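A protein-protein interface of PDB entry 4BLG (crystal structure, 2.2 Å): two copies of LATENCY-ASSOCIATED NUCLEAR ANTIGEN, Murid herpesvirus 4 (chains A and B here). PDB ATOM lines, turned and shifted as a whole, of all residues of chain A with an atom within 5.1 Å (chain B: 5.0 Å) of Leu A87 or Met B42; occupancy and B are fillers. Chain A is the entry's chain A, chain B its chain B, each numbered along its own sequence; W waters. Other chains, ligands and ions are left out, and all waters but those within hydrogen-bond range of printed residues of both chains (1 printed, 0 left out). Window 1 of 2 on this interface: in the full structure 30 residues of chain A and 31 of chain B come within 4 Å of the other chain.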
ATOM      1  N   ALA A  40     -20.750  -6.178 -27.603  1.00  0.00           N
ATOM      2  CA  ALA A  40     -20.581  -4.879 -26.994  1.00  0.00           C
ATOM      3  C   ALA A  40     -19.252  -4.303 -27.427  1.00  0.00           C
ATOM      4  O   ALA A  40     -18.418  -4.995 -28.012  1.00  0.00           O
ATOM      5  CB  ALA A  40     -20.638  -4.989 -25.485  1.00  0.00           C
ATOM      6  N   VAL A  41     -19.066  -3.022 -27.162  1.00  0.00           N
ATOM      7  CA  VAL A  41     -17.750  -2.436 -27.258  1.00  0.00           C
ATOM      8  C   VAL A  41     -17.379  -1.936 -25.878  1.00  0.00           C
ATOM      9  O   VAL A  41     -18.138  -1.200 -25.241  1.00  0.00           O
ATOM     10  CB  VAL A  41     -17.696  -1.273 -28.264  1.00  0.00           C
ATOM     11  CG1 VAL A  41     -16.261  -0.774 -28.407  1.00  0.00           C
ATOM     12  CG2 VAL A  41     -18.245  -1.708 -29.619  1.00  0.00           C
ATOM     13  N   MET A  42     -16.227  -2.369 -25.393  1.00  0.00           N
ATOM     14  CA  MET A  42     -15.653  -1.774 -24.202  1.00  0.00           C
ATOM     15  C   MET A  42     -14.858  -0.548 -24.613  1.00  0.00           C
ATOM     16  O   MET A  42     -13.881  -0.653 -25.357  1.00  0.00           O
ATOM     17  CB  MET A  42     -14.739  -2.767 -23.483  1.00  0.00           C
ATOM     18  CG  MET A  42     -14.125  -2.191 -22.203  1.00  0.00           C
ATOM     19  SD  MET A  42     -13.062  -3.359 -21.340  1.00  0.00           S
ATOM     20  CE  MET A  42     -14.299  -4.389 -20.544  1.00  0.00           C
ATOM     21  N   LEU A  64     -26.926   0.323 -25.721  1.00  0.00           N
ATOM     22  CA  LEU A  64     -27.121   0.627 -24.312  1.00  0.00           C
ATOM     23  C   LEU A  64     -25.778   0.587 -23.616  1.00  0.00           C
ATOM     24  O   LEU A  64     -25.028  -0.376 -23.761  1.00  0.00           O
ATOM     25  CB  LEU A  64     -28.069  -0.378 -23.675  1.00  0.00           C
ATOM     26  CG  LEU A  64     -29.356  -0.667 -24.457  1.00  0.00           C
ATOM     27  CD1 LEU A  64     -30.170  -1.718 -23.728  1.00  0.00           C
ATOM     28  CD2 LEU A  64     -30.185   0.582 -24.658  1.00  0.00           C
ATOM     29  N   SER A  65     -25.466   1.632 -22.859  1.00  0.00           N
ATOM     30  CA  SER A  65     -24.183   1.690 -22.180  1.00  0.00           C
ATOM     31  C   SER A  65     -24.310   1.702 -20.666  1.00  0.00           C
ATOM     32  O   SER A  65     -25.201   2.325 -20.093  1.00  0.00           O
ATOM     33  CB  SER A  65     -23.370   2.897 -22.639  1.00  0.00           C
ATOM     34  OG  SER A  65     -23.030   2.788 -24.009  1.00  0.00           O
ATOM     35  N   THR A  66     -23.392   0.986 -20.037  1.00  0.00           N
ATOM     36  CA  THR A  66     -23.282   0.945 -18.597  1.00  0.00           C
ATOM     37  C   THR A  66     -22.745   2.272 -18.089  1.00  0.00           C
ATOM     38  O   THR A  66     -22.200   3.065 -18.865  1.00  0.00           O
ATOM     39  CB  THR A  66     -22.270  -0.113 -18.180  1.00  0.00           C
ATOM     40  OG1 THR A  66     -20.979   0.257 -18.683  1.00  0.00           O
ATOM     41  CG2 THR A  66     -22.652  -1.458 -18.730  1.00  0.00           C
ATOM     42  N   TYR A  85     -13.584   2.223 -17.687  1.00  0.00           N
ATOM     43  CA  TYR A  85     -14.221   1.609 -18.846  1.00  0.00           C
ATOM     44  C   TYR A  85     -15.723   1.730 -18.767  1.00  0.00           C
ATOM     45  O   TYR A  85     -16.275   2.029 -17.725  1.00  0.00           O
ATOM     46  CB  TYR A  85     -13.864   0.123 -18.952  1.00  0.00           C
ATOM     47  CG  TYR A  85     -14.727  -0.772 -18.083  1.00  0.00           C
ATOM     48  CD1 TYR A  85     -14.375  -1.048 -16.765  1.00  0.00           C
ATOM     49  CD2 TYR A  85     -15.894  -1.344 -18.582  1.00  0.00           C
ATOM     50  CE1 TYR A  85     -15.167  -1.869 -15.966  1.00  0.00           C
ATOM     51  CE2 TYR A  85     -16.685  -2.167 -17.794  1.00  0.00           C
ATOM     52  CZ  TYR A  85     -16.319  -2.424 -16.488  1.00  0.00           C
ATOM     53  OH  TYR A  85     -17.109  -3.242 -15.708  1.00  0.00           O
ATOM     54  N   LEU A  86     -16.378   1.493 -19.893  1.00  0.00           N
ATOM     55  CA  LEU A  86     -17.805   1.249 -19.907  1.00  0.00           C
ATOM     56  C   LEU A  86     -18.070   0.293 -21.047  1.00  0.00           C
ATOM     57  O   LEU A  86     -17.227   0.109 -21.918  1.00  0.00           O
ATOM     58  CB  LEU A  86     -18.613   2.541 -20.071  1.00  0.00           C
ATOM     59  CG  LEU A  86     -18.445   3.378 -21.344  1.00  0.00           C
ATOM     60  CD1 LEU A  86     -19.053   2.710 -22.562  1.00  0.00           C
ATOM     61  CD2 LEU A  86     -19.090   4.735 -21.132  1.00  0.00           C
ATOM     62  N   LEU A  87     -19.238  -0.329 -21.010  1.00  0.00           N
ATOM     63  CA  LEU A  87     -19.657  -1.274 -22.025  1.00  0.00           C
ATOM     64  C   LEU A  87     -20.856  -0.712 -22.755  1.00  0.00           C
ATOM     65  O   LEU A  87     -21.774  -0.193 -22.130  1.00  0.00           O
ATOM     66  CB  LEU A  87     -20.050  -2.601 -21.376  1.00  0.00           C
ATOM     67  CG  LEU A  87     -18.906  -3.433 -20.804  1.00  0.00           C
ATOM     68  CD1 LEU A  87     -19.466  -4.645 -20.078  1.00  0.00           C
ATOM     69  CD2 LEU A  87     -17.969  -3.856 -21.916  1.00  0.00           C
ATOM     70  N   SER A  88     -20.842  -0.822 -24.077  1.00  0.00           N
ATOM     71  CA  SER A  88     -21.956  -0.374 -24.895  1.00  0.00           C
ATOM     72  C   SER A  88     -22.457  -1.597 -25.606  1.00  0.00           C
ATOM     73  O   SER A  88     -21.777  -2.124 -26.482  1.00  0.00           O
ATOM     74  CB  SER A  88     -21.514   0.681 -25.917  1.00  0.00           C
ATOM     75  OG  SER A  88     -20.906   1.794 -25.291  1.00  0.00           O
ATOM     76  N   PHE A  89     -23.641  -2.058 -25.218  1.00  0.00           N
ATOM     77  CA  PHE A  89     -24.190  -3.298 -25.747  1.00  0.00           C
ATOM     78  C   PHE A  89     -24.947  -3.065 -27.050  1.00  0.00           C
ATOM     79  O   PHE A  89     -25.665  -2.075 -27.187  1.00  0.00           O
ATOM     80  CB  PHE A  89     -25.116  -3.939 -24.716  1.00  0.00           C
ATOM     81  CG  PHE A  89     -24.439  -4.251 -23.416  1.00  0.00           C
ATOM     82  CD1 PHE A  89     -23.722  -5.427 -23.259  1.00  0.00           C
ATOM     83  CD2 PHE A  89     -24.515  -3.372 -22.351  1.00  0.00           C
ATOM     84  CE1 PHE A  89     -23.084  -5.716 -22.059  1.00  0.00           C
ATOM     85  CE2 PHE A  89     -23.882  -3.654 -21.153  1.00  0.00           C
ATOM     86  CZ  PHE A  89     -23.170  -4.831 -21.005  1.00  0.00           C
ATOM     87  N   VAL A 119     -16.212  -6.976 -27.955  1.00  0.00           N
ATOM     88  CA  VAL A 119     -16.486  -8.028 -26.993  1.00  0.00           C
ATOM     89  C   VAL A 119     -17.707  -8.807 -27.453  1.00  0.00           C
ATOM     90  O   VAL A 119     -18.598  -8.247 -28.081  1.00  0.00           O
ATOM     91  CB  VAL A 119     -16.767  -7.446 -25.592  1.00  0.00           C
ATOM     92  CG1 VAL A 119     -17.075  -8.556 -24.606  1.00  0.00           C
ATOM     93  CG2 VAL A 119     -15.584  -6.632 -25.113  1.00  0.00           C
ATOM     94  N   PHE A 125     -25.484 -11.255 -23.794  1.00  0.00           N
ATOM     95  CA  PHE A 125     -25.327 -10.644 -22.485  1.00  0.00           C
ATOM     96  C   PHE A 125     -26.620 -10.759 -21.694  1.00  0.00           C
ATOM     97  O   PHE A 125     -27.703 -10.807 -22.275  1.00  0.00           O
ATOM     98  CB  PHE A 125     -24.887  -9.196 -22.623  1.00  0.00           C
ATOM     99  CG  PHE A 125     -23.445  -9.044 -23.012  1.00  0.00           C
ATOM    100  CD1 PHE A 125     -22.448  -9.163 -22.062  1.00  0.00           C
ATOM    101  CD2 PHE A 125     -23.087  -8.788 -24.317  1.00  0.00           C
ATOM    102  CE1 PHE A 125     -21.125  -9.026 -22.406  1.00  0.00           C
ATOM    103  CE2 PHE A 125     -21.757  -8.649 -24.667  1.00  0.00           C
ATOM    104  CZ  PHE A 125     -20.778  -8.774 -23.710  1.00  0.00           C
ATOM    105  N   PRO A 126     -26.507 -10.822 -20.357  1.00  0.00           N
ATOM    106  CA  PRO A 126     -27.648 -11.092 -19.479  1.00  0.00           C
ATOM    107  C   PRO A 126     -28.548  -9.873 -19.276  1.00  0.00           C
ATOM    108  O   PRO A 126     -28.794  -9.471 -18.144  1.00  0.00           O
ATOM    109  CB  PRO A 126     -26.975 -11.490 -18.167  1.00  0.00           C
ATOM    110  CG  PRO A 126     -25.710 -10.691 -18.162  1.00  0.00           C
ATOM    111  CD  PRO A 126     -25.265 -10.607 -19.592  1.00  0.00           C
ATOM    112  N   ALA B  40     -13.371 -13.512 -20.034  1.00  0.00           N
ATOM    113  CA  ALA B  40     -13.864 -13.176 -18.708  1.00  0.00           C
ATOM    114  C   ALA B  40     -15.188 -13.866 -18.471  1.00  0.00           C
ATOM    115  O   ALA B  40     -15.782 -14.425 -19.395  1.00  0.00           O
ATOM    116  CB  ALA B  40     -14.019 -11.679 -18.552  1.00  0.00           C
ATOM    117  N   VAL B  41     -15.626 -13.861 -17.219  1.00  0.00           N
ATOM    118  CA  VAL B  41     -16.983 -14.251 -16.889  1.00  0.00           C
ATOM    119  C   VAL B  41     -17.686 -13.026 -16.335  1.00  0.00           C
ATOM    120  O   VAL B  41     -17.197 -12.372 -15.402  1.00  0.00           O
ATOM    121  CB  VAL B  41     -17.045 -15.376 -15.832  1.00  0.00           C
ATOM    122  CG1 VAL B  41     -18.486 -15.819 -15.612  1.00  0.00           C
ATOM    123  CG2 VAL B  41     -16.201 -16.562 -16.245  1.00  0.00           C
ATOM    124  N   MET B  42     -18.825 -12.685 -16.912  1.00  0.00           N
ATOM    125  CA  MET B  42     -19.664 -11.676 -16.294  1.00  0.00           C
ATOM    126  C   MET B  42     -20.589 -12.365 -15.311  1.00  0.00           C
ATOM    127  O   MET B  42     -21.369 -13.240 -15.685  1.00  0.00           O
ATOM    128  CB  MET B  42     -20.478 -10.920 -17.338  1.00  0.00           C
ATOM    129  CG  MET B  42     -21.430  -9.909 -16.731  1.00  0.00           C
ATOM    130  SD  MET B  42     -22.378  -9.010 -17.967  1.00  0.00           S
ATOM    131  CE  MET B  42     -21.129  -7.936 -18.664  1.00  0.00           C
ATOM    132  N   PHE B  43     -20.495 -11.966 -14.050  1.00  0.00           N
ATOM    133  CA  PHE B  43     -21.403 -12.469 -13.034  1.00  0.00           C
ATOM    134  C   PHE B  43     -22.445 -11.400 -12.781  1.00  0.00           C
ATOM    135  O   PHE B  43     -22.093 -10.256 -12.538  1.00  0.00           O
ATOM    136  CB  PHE B  43     -20.651 -12.801 -11.746  1.00  0.00           C
ATOM    137  CG  PHE B  43     -19.721 -13.971 -11.880  1.00  0.00           C
ATOM    138  CD1 PHE B  43     -20.213 -15.270 -11.866  1.00  0.00           C
ATOM    139  CD2 PHE B  43     -18.359 -13.775 -12.015  1.00  0.00           C
ATOM    140  CE1 PHE B  43     -19.364 -16.350 -11.992  1.00  0.00           C
ATOM    141  CE2 PHE B  43     -17.498 -14.857 -12.141  1.00  0.00           C
ATOM    142  CZ  PHE B  43     -17.999 -16.142 -12.128  1.00  0.00           C
ATOM    143  N   SER B  44     -23.721 -11.772 -12.838  1.00  0.00           N
ATOM    144  CA  SER B  44     -24.802 -10.802 -12.701  1.00  0.00           C
ATOM    145  C   SER B  44     -25.841 -11.244 -11.691  1.00  0.00           C
ATOM    146  O   SER B  44     -26.007 -12.431 -11.432  1.00  0.00           O
ATOM    147  CB  SER B  44     -25.485 -10.532 -14.047  1.00  0.00           C
ATOM    148  OG  SER B  44     -25.856 -11.732 -14.708  1.00  0.00           O
ATOM    149  N   LEU B  71     -26.048  -2.900 -15.097  1.00  0.00           N
ATOM    150  CA  LEU B  71     -26.377  -2.997 -16.513  1.00  0.00           C
ATOM    151  C   LEU B  71     -27.451  -1.956 -16.809  1.00  0.00           C
ATOM    152  O   LEU B  71     -28.254  -1.622 -15.939  1.00  0.00           O
ATOM    153  CB  LEU B  71     -26.882  -4.392 -16.880  1.00  0.00           C
ATOM    154  CG  LEU B  71     -25.916  -5.567 -16.716  1.00  0.00           C
ATOM    155  CD1 LEU B  71     -26.646  -6.871 -16.986  1.00  0.00           C
ATOM    156  CD2 LEU B  71     -24.718  -5.439 -17.634  1.00  0.00           C
ATOM    157  N   TYR B  85     -23.650  -6.305 -12.114  1.00  0.00           N
ATOM    158  CA  TYR B  85     -22.717  -7.233 -12.725  1.00  0.00           C
ATOM    159  C   TYR B  85     -21.299  -6.875 -12.328  1.00  0.00           C
ATOM    160  O   TYR B  85     -21.031  -5.767 -11.884  1.00  0.00           O
ATOM    161  CB  TYR B  85     -22.807  -7.167 -14.248  1.00  0.00           C
ATOM    162  CG  TYR B  85     -22.001  -6.031 -14.837  1.00  0.00           C
ATOM    163  CD1 TYR B  85     -22.553  -4.769 -14.990  1.00  0.00           C
ATOM    164  CD2 TYR B  85     -20.681  -6.225 -15.232  1.00  0.00           C
ATOM    165  CE1 TYR B  85     -21.812  -3.726 -15.523  1.00  0.00           C
ATOM    166  CE2 TYR B  85     -19.937  -5.200 -15.761  1.00  0.00           C
ATOM    167  CZ  TYR B  85     -20.501  -3.948 -15.904  1.00  0.00           C
ATOM    168  OH  TYR B  85     -19.753  -2.928 -16.438  1.00  0.00           O
ATOM    169  N   LEU B  86     -20.402  -7.839 -12.485  1.00  0.00           N
ATOM    170  CA  LEU B  86     -18.980  -7.574 -12.508  1.00  0.00           C
ATOM    171  C   LEU B  86     -18.366  -8.485 -13.560  1.00  0.00           C
ATOM    172  O   LEU B  86     -19.019  -9.402 -14.044  1.00  0.00           O
ATOM    173  CB  LEU B  86     -18.331  -7.794 -11.144  1.00  0.00           C
ATOM    174  CG  LEU B  86     -18.386  -9.173 -10.491  1.00  0.00           C
ATOM    175  CD1 LEU B  86     -17.493 -10.178 -11.198  1.00  0.00           C
ATOM    176  CD2 LEU B  86     -17.956  -9.033  -9.050  1.00  0.00           C
ATOM    177  N   LEU B  87     -17.115  -8.205 -13.907  1.00  0.00           N
ATOM    178  CA  LEU B  87     -16.352  -8.997 -14.849  1.00  0.00           C
ATOM    179  C   LEU B  87     -15.136  -9.569 -14.151  1.00  0.00           C
ATOM    180  O   LEU B  87     -14.457  -8.863 -13.404  1.00  0.00           O
ATOM    181  CB  LEU B  87     -15.885  -8.114 -16.003  1.00  0.00           C
ATOM    182  CG  LEU B  87     -16.959  -7.690 -17.005  1.00  0.00           C
ATOM    183  CD1 LEU B  87     -16.442  -6.550 -17.868  1.00  0.00           C
ATOM    184  CD2 LEU B  87     -17.361  -8.875 -17.859  1.00  0.00           C
ATOM    185  N   GLU B 115     -25.860 -15.371 -11.761  1.00  0.00           N
ATOM    186  CA  GLU B 115     -25.689 -15.966 -13.071  1.00  0.00           C
ATOM    187  C   GLU B 115     -24.311 -15.608 -13.622  1.00  0.00           C
ATOM    188  O   GLU B 115     -23.719 -14.611 -13.254  1.00  0.00           O
ATOM    189  CB  GLU B 115     -26.786 -15.463 -14.008  1.00  0.00           C
ATOM    190  CG  GLU B 115     -28.184 -15.810 -13.543  1.00  0.00           C
ATOM    191  CD  GLU B 115     -29.249 -15.404 -14.548  1.00  0.00           C
ATOM    192  OE1 GLU B 115     -28.893 -15.046 -15.693  1.00  0.00           O
ATOM    193  OE2 GLU B 115     -30.445 -15.442 -14.184  1.00  0.00           O
ATOM    194  N   GLY B 116     -23.799 -16.445 -14.505  1.00  0.00           N
ATOM    195  CA  GLY B 116     -22.498 -16.222 -15.095  1.00  0.00           C
ATOM    196  C   GLY B 116     -22.595 -16.394 -16.591  1.00  0.00           C
ATOM    197  O   GLY B 116     -23.300 -17.269 -17.078  1.00  0.00           O
ATOM    198  N   THR B 117     -21.887 -15.545 -17.320  1.00  0.00           N
ATOM    199  CA  THR B 117     -21.937 -15.545 -18.773  1.00  0.00           C
ATOM    200  C   THR B 117     -20.512 -15.469 -19.278  1.00  0.00           C
ATOM    201  O   THR B 117     -19.760 -14.611 -18.855  1.00  0.00           O
ATOM    202  CB  THR B 117     -22.726 -14.326 -19.282  1.00  0.00           C
ATOM    203  OG1 THR B 117     -24.025 -14.315 -18.678  1.00  0.00           O
ATOM    204  CG2 THR B 117     -22.865 -14.341 -20.808  1.00  0.00           C
ATOM    205  N   VAL B 119     -17.576 -14.501 -21.709  1.00  0.00           N
ATOM    206  CA  VAL B 119     -17.362 -13.319 -22.518  1.00  0.00           C
ATOM    207  C   VAL B 119     -15.962 -13.387 -23.101  1.00  0.00           C
ATOM    208  O   VAL B 119     -15.052 -13.928 -22.475  1.00  0.00           O
ATOM    209  CB  VAL B 119     -17.495 -12.033 -21.666  1.00  0.00           C
ATOM    210  CG1 VAL B 119     -17.055 -10.830 -22.457  1.00  0.00           C
ATOM    211  CG2 VAL B 119     -18.924 -11.860 -21.191  1.00  0.00           C
HETATM  212  O   HOH W   1     -19.893  -0.283 -15.493  1.00  0.00           O
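Leu A87 touches one residue of chain B.
Printed residues of chain B within 4 Å of Phe A125: Met B42 (3.8 Å) and Val B119 (3.8 Å).
Printed residues of chain A within 4 Å of Leu B71: Phe A89 and Pro A126.
Of the printed residues of chain B, Pro A126 touches Met B42, Ser B44 and Leu B71.
Printed residues of chain B within 4 Å of Phe A89: Leu B71 (3.8 Å).
Printed residues of chain A within 4 Å of Ser B44: Pro A126 (3.6 Å).
The nearest residue of chain A that does not touch Met B42 is Phe A89 (4.4 Å).
Tyr B85 touches Thr A66 (OH to CG2, 3.98 Å).
Met B42 touches Leu A87 (CE to CD1, 3.9 Å).
Phe A89 touches Leu B71 (CZ to CD2, 3.8 Å).
CG1 of Val A119 touches CG1 of Val B119, 3.1 Å away.
Phe A125 touches Met B42 (CD1 to CE, 3.8 Å).
Phe A125 touches Val B119 (CE1 to CG2, 3.8 Å).
Pro A126 touches Met B42.
Pro A126 touches Ser B44.
CD1 of Leu B71 touches O of Pro A126, at 3.6 Å.
Of the 14 printed residues of chain A, 7 touch a printed residue of chain B.
Hydrophobic or aromatic side chains of chain A within 4 Å of the printed part of chain B: Tyr A85, Leu A87, Phe A89, Val A119, Phe A125 and Pro A126.
Along chain A the printed residues that touch a printed residue of chain B span positions 66 to 126.
Hydrophobic or aromatic side chains of chain B that line the printed part of chain A: Met B42, Leu B71, Tyr B85 and Val B119.
Among the printed residues, 10 pairs touch across the chains.
Among the printed residues, no Asp or Glu carboxylate lies within 4 Å of a Lys or Arg side-chain nitrogen of the other chain.
Water W1 bridges the side-chain hydroxyl (OH) of Tyr B85 (2.8 Å) and the side-chain hydroxyl (OG1) of Thr A66 (3.4 Å).
The backbone carbonyl oxygen (O) of Ala B40 sits at hydrogen-bond distance from the backbone NH (N) of Val B119 (2.9 Å).
N of Phe A89 is in hydrogen-bond range of O of Leu A64.
The backbone carbonyl oxygen (O) of Leu A87 sits at hydrogen-bond distance from the backbone NH (N) of Thr A66 (2.9 Å).
N of Val A119 sits at hydrogen-bond distance from O of Ala A40 (3.0 Å).
The backbone carbonyl oxygen of Met B42 lies within hydrogen-bond range of the backbone NH of Thr B117, at 2.9 Å.
N of Ser B44 lies within hydrogen-bond range of O of Glu B115.
Tyr A85 touches its own counterpart, Tyr B85.
Leu A87 touches Met B42, but with the chains exchanged Met A42 does not touch Leu B87 (4.1 Å).
Val B119 touches its own counterpart, Val A119.
Positions printed for both chains: 40, 41, 42, 85, 86, 87 and 119.
The side-chain hydroxyl (OH) of Tyr A85 is in hydrogen-bond range of the side-chain hydroxyl (OH) of Tyr B85, 2.8 Å away.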
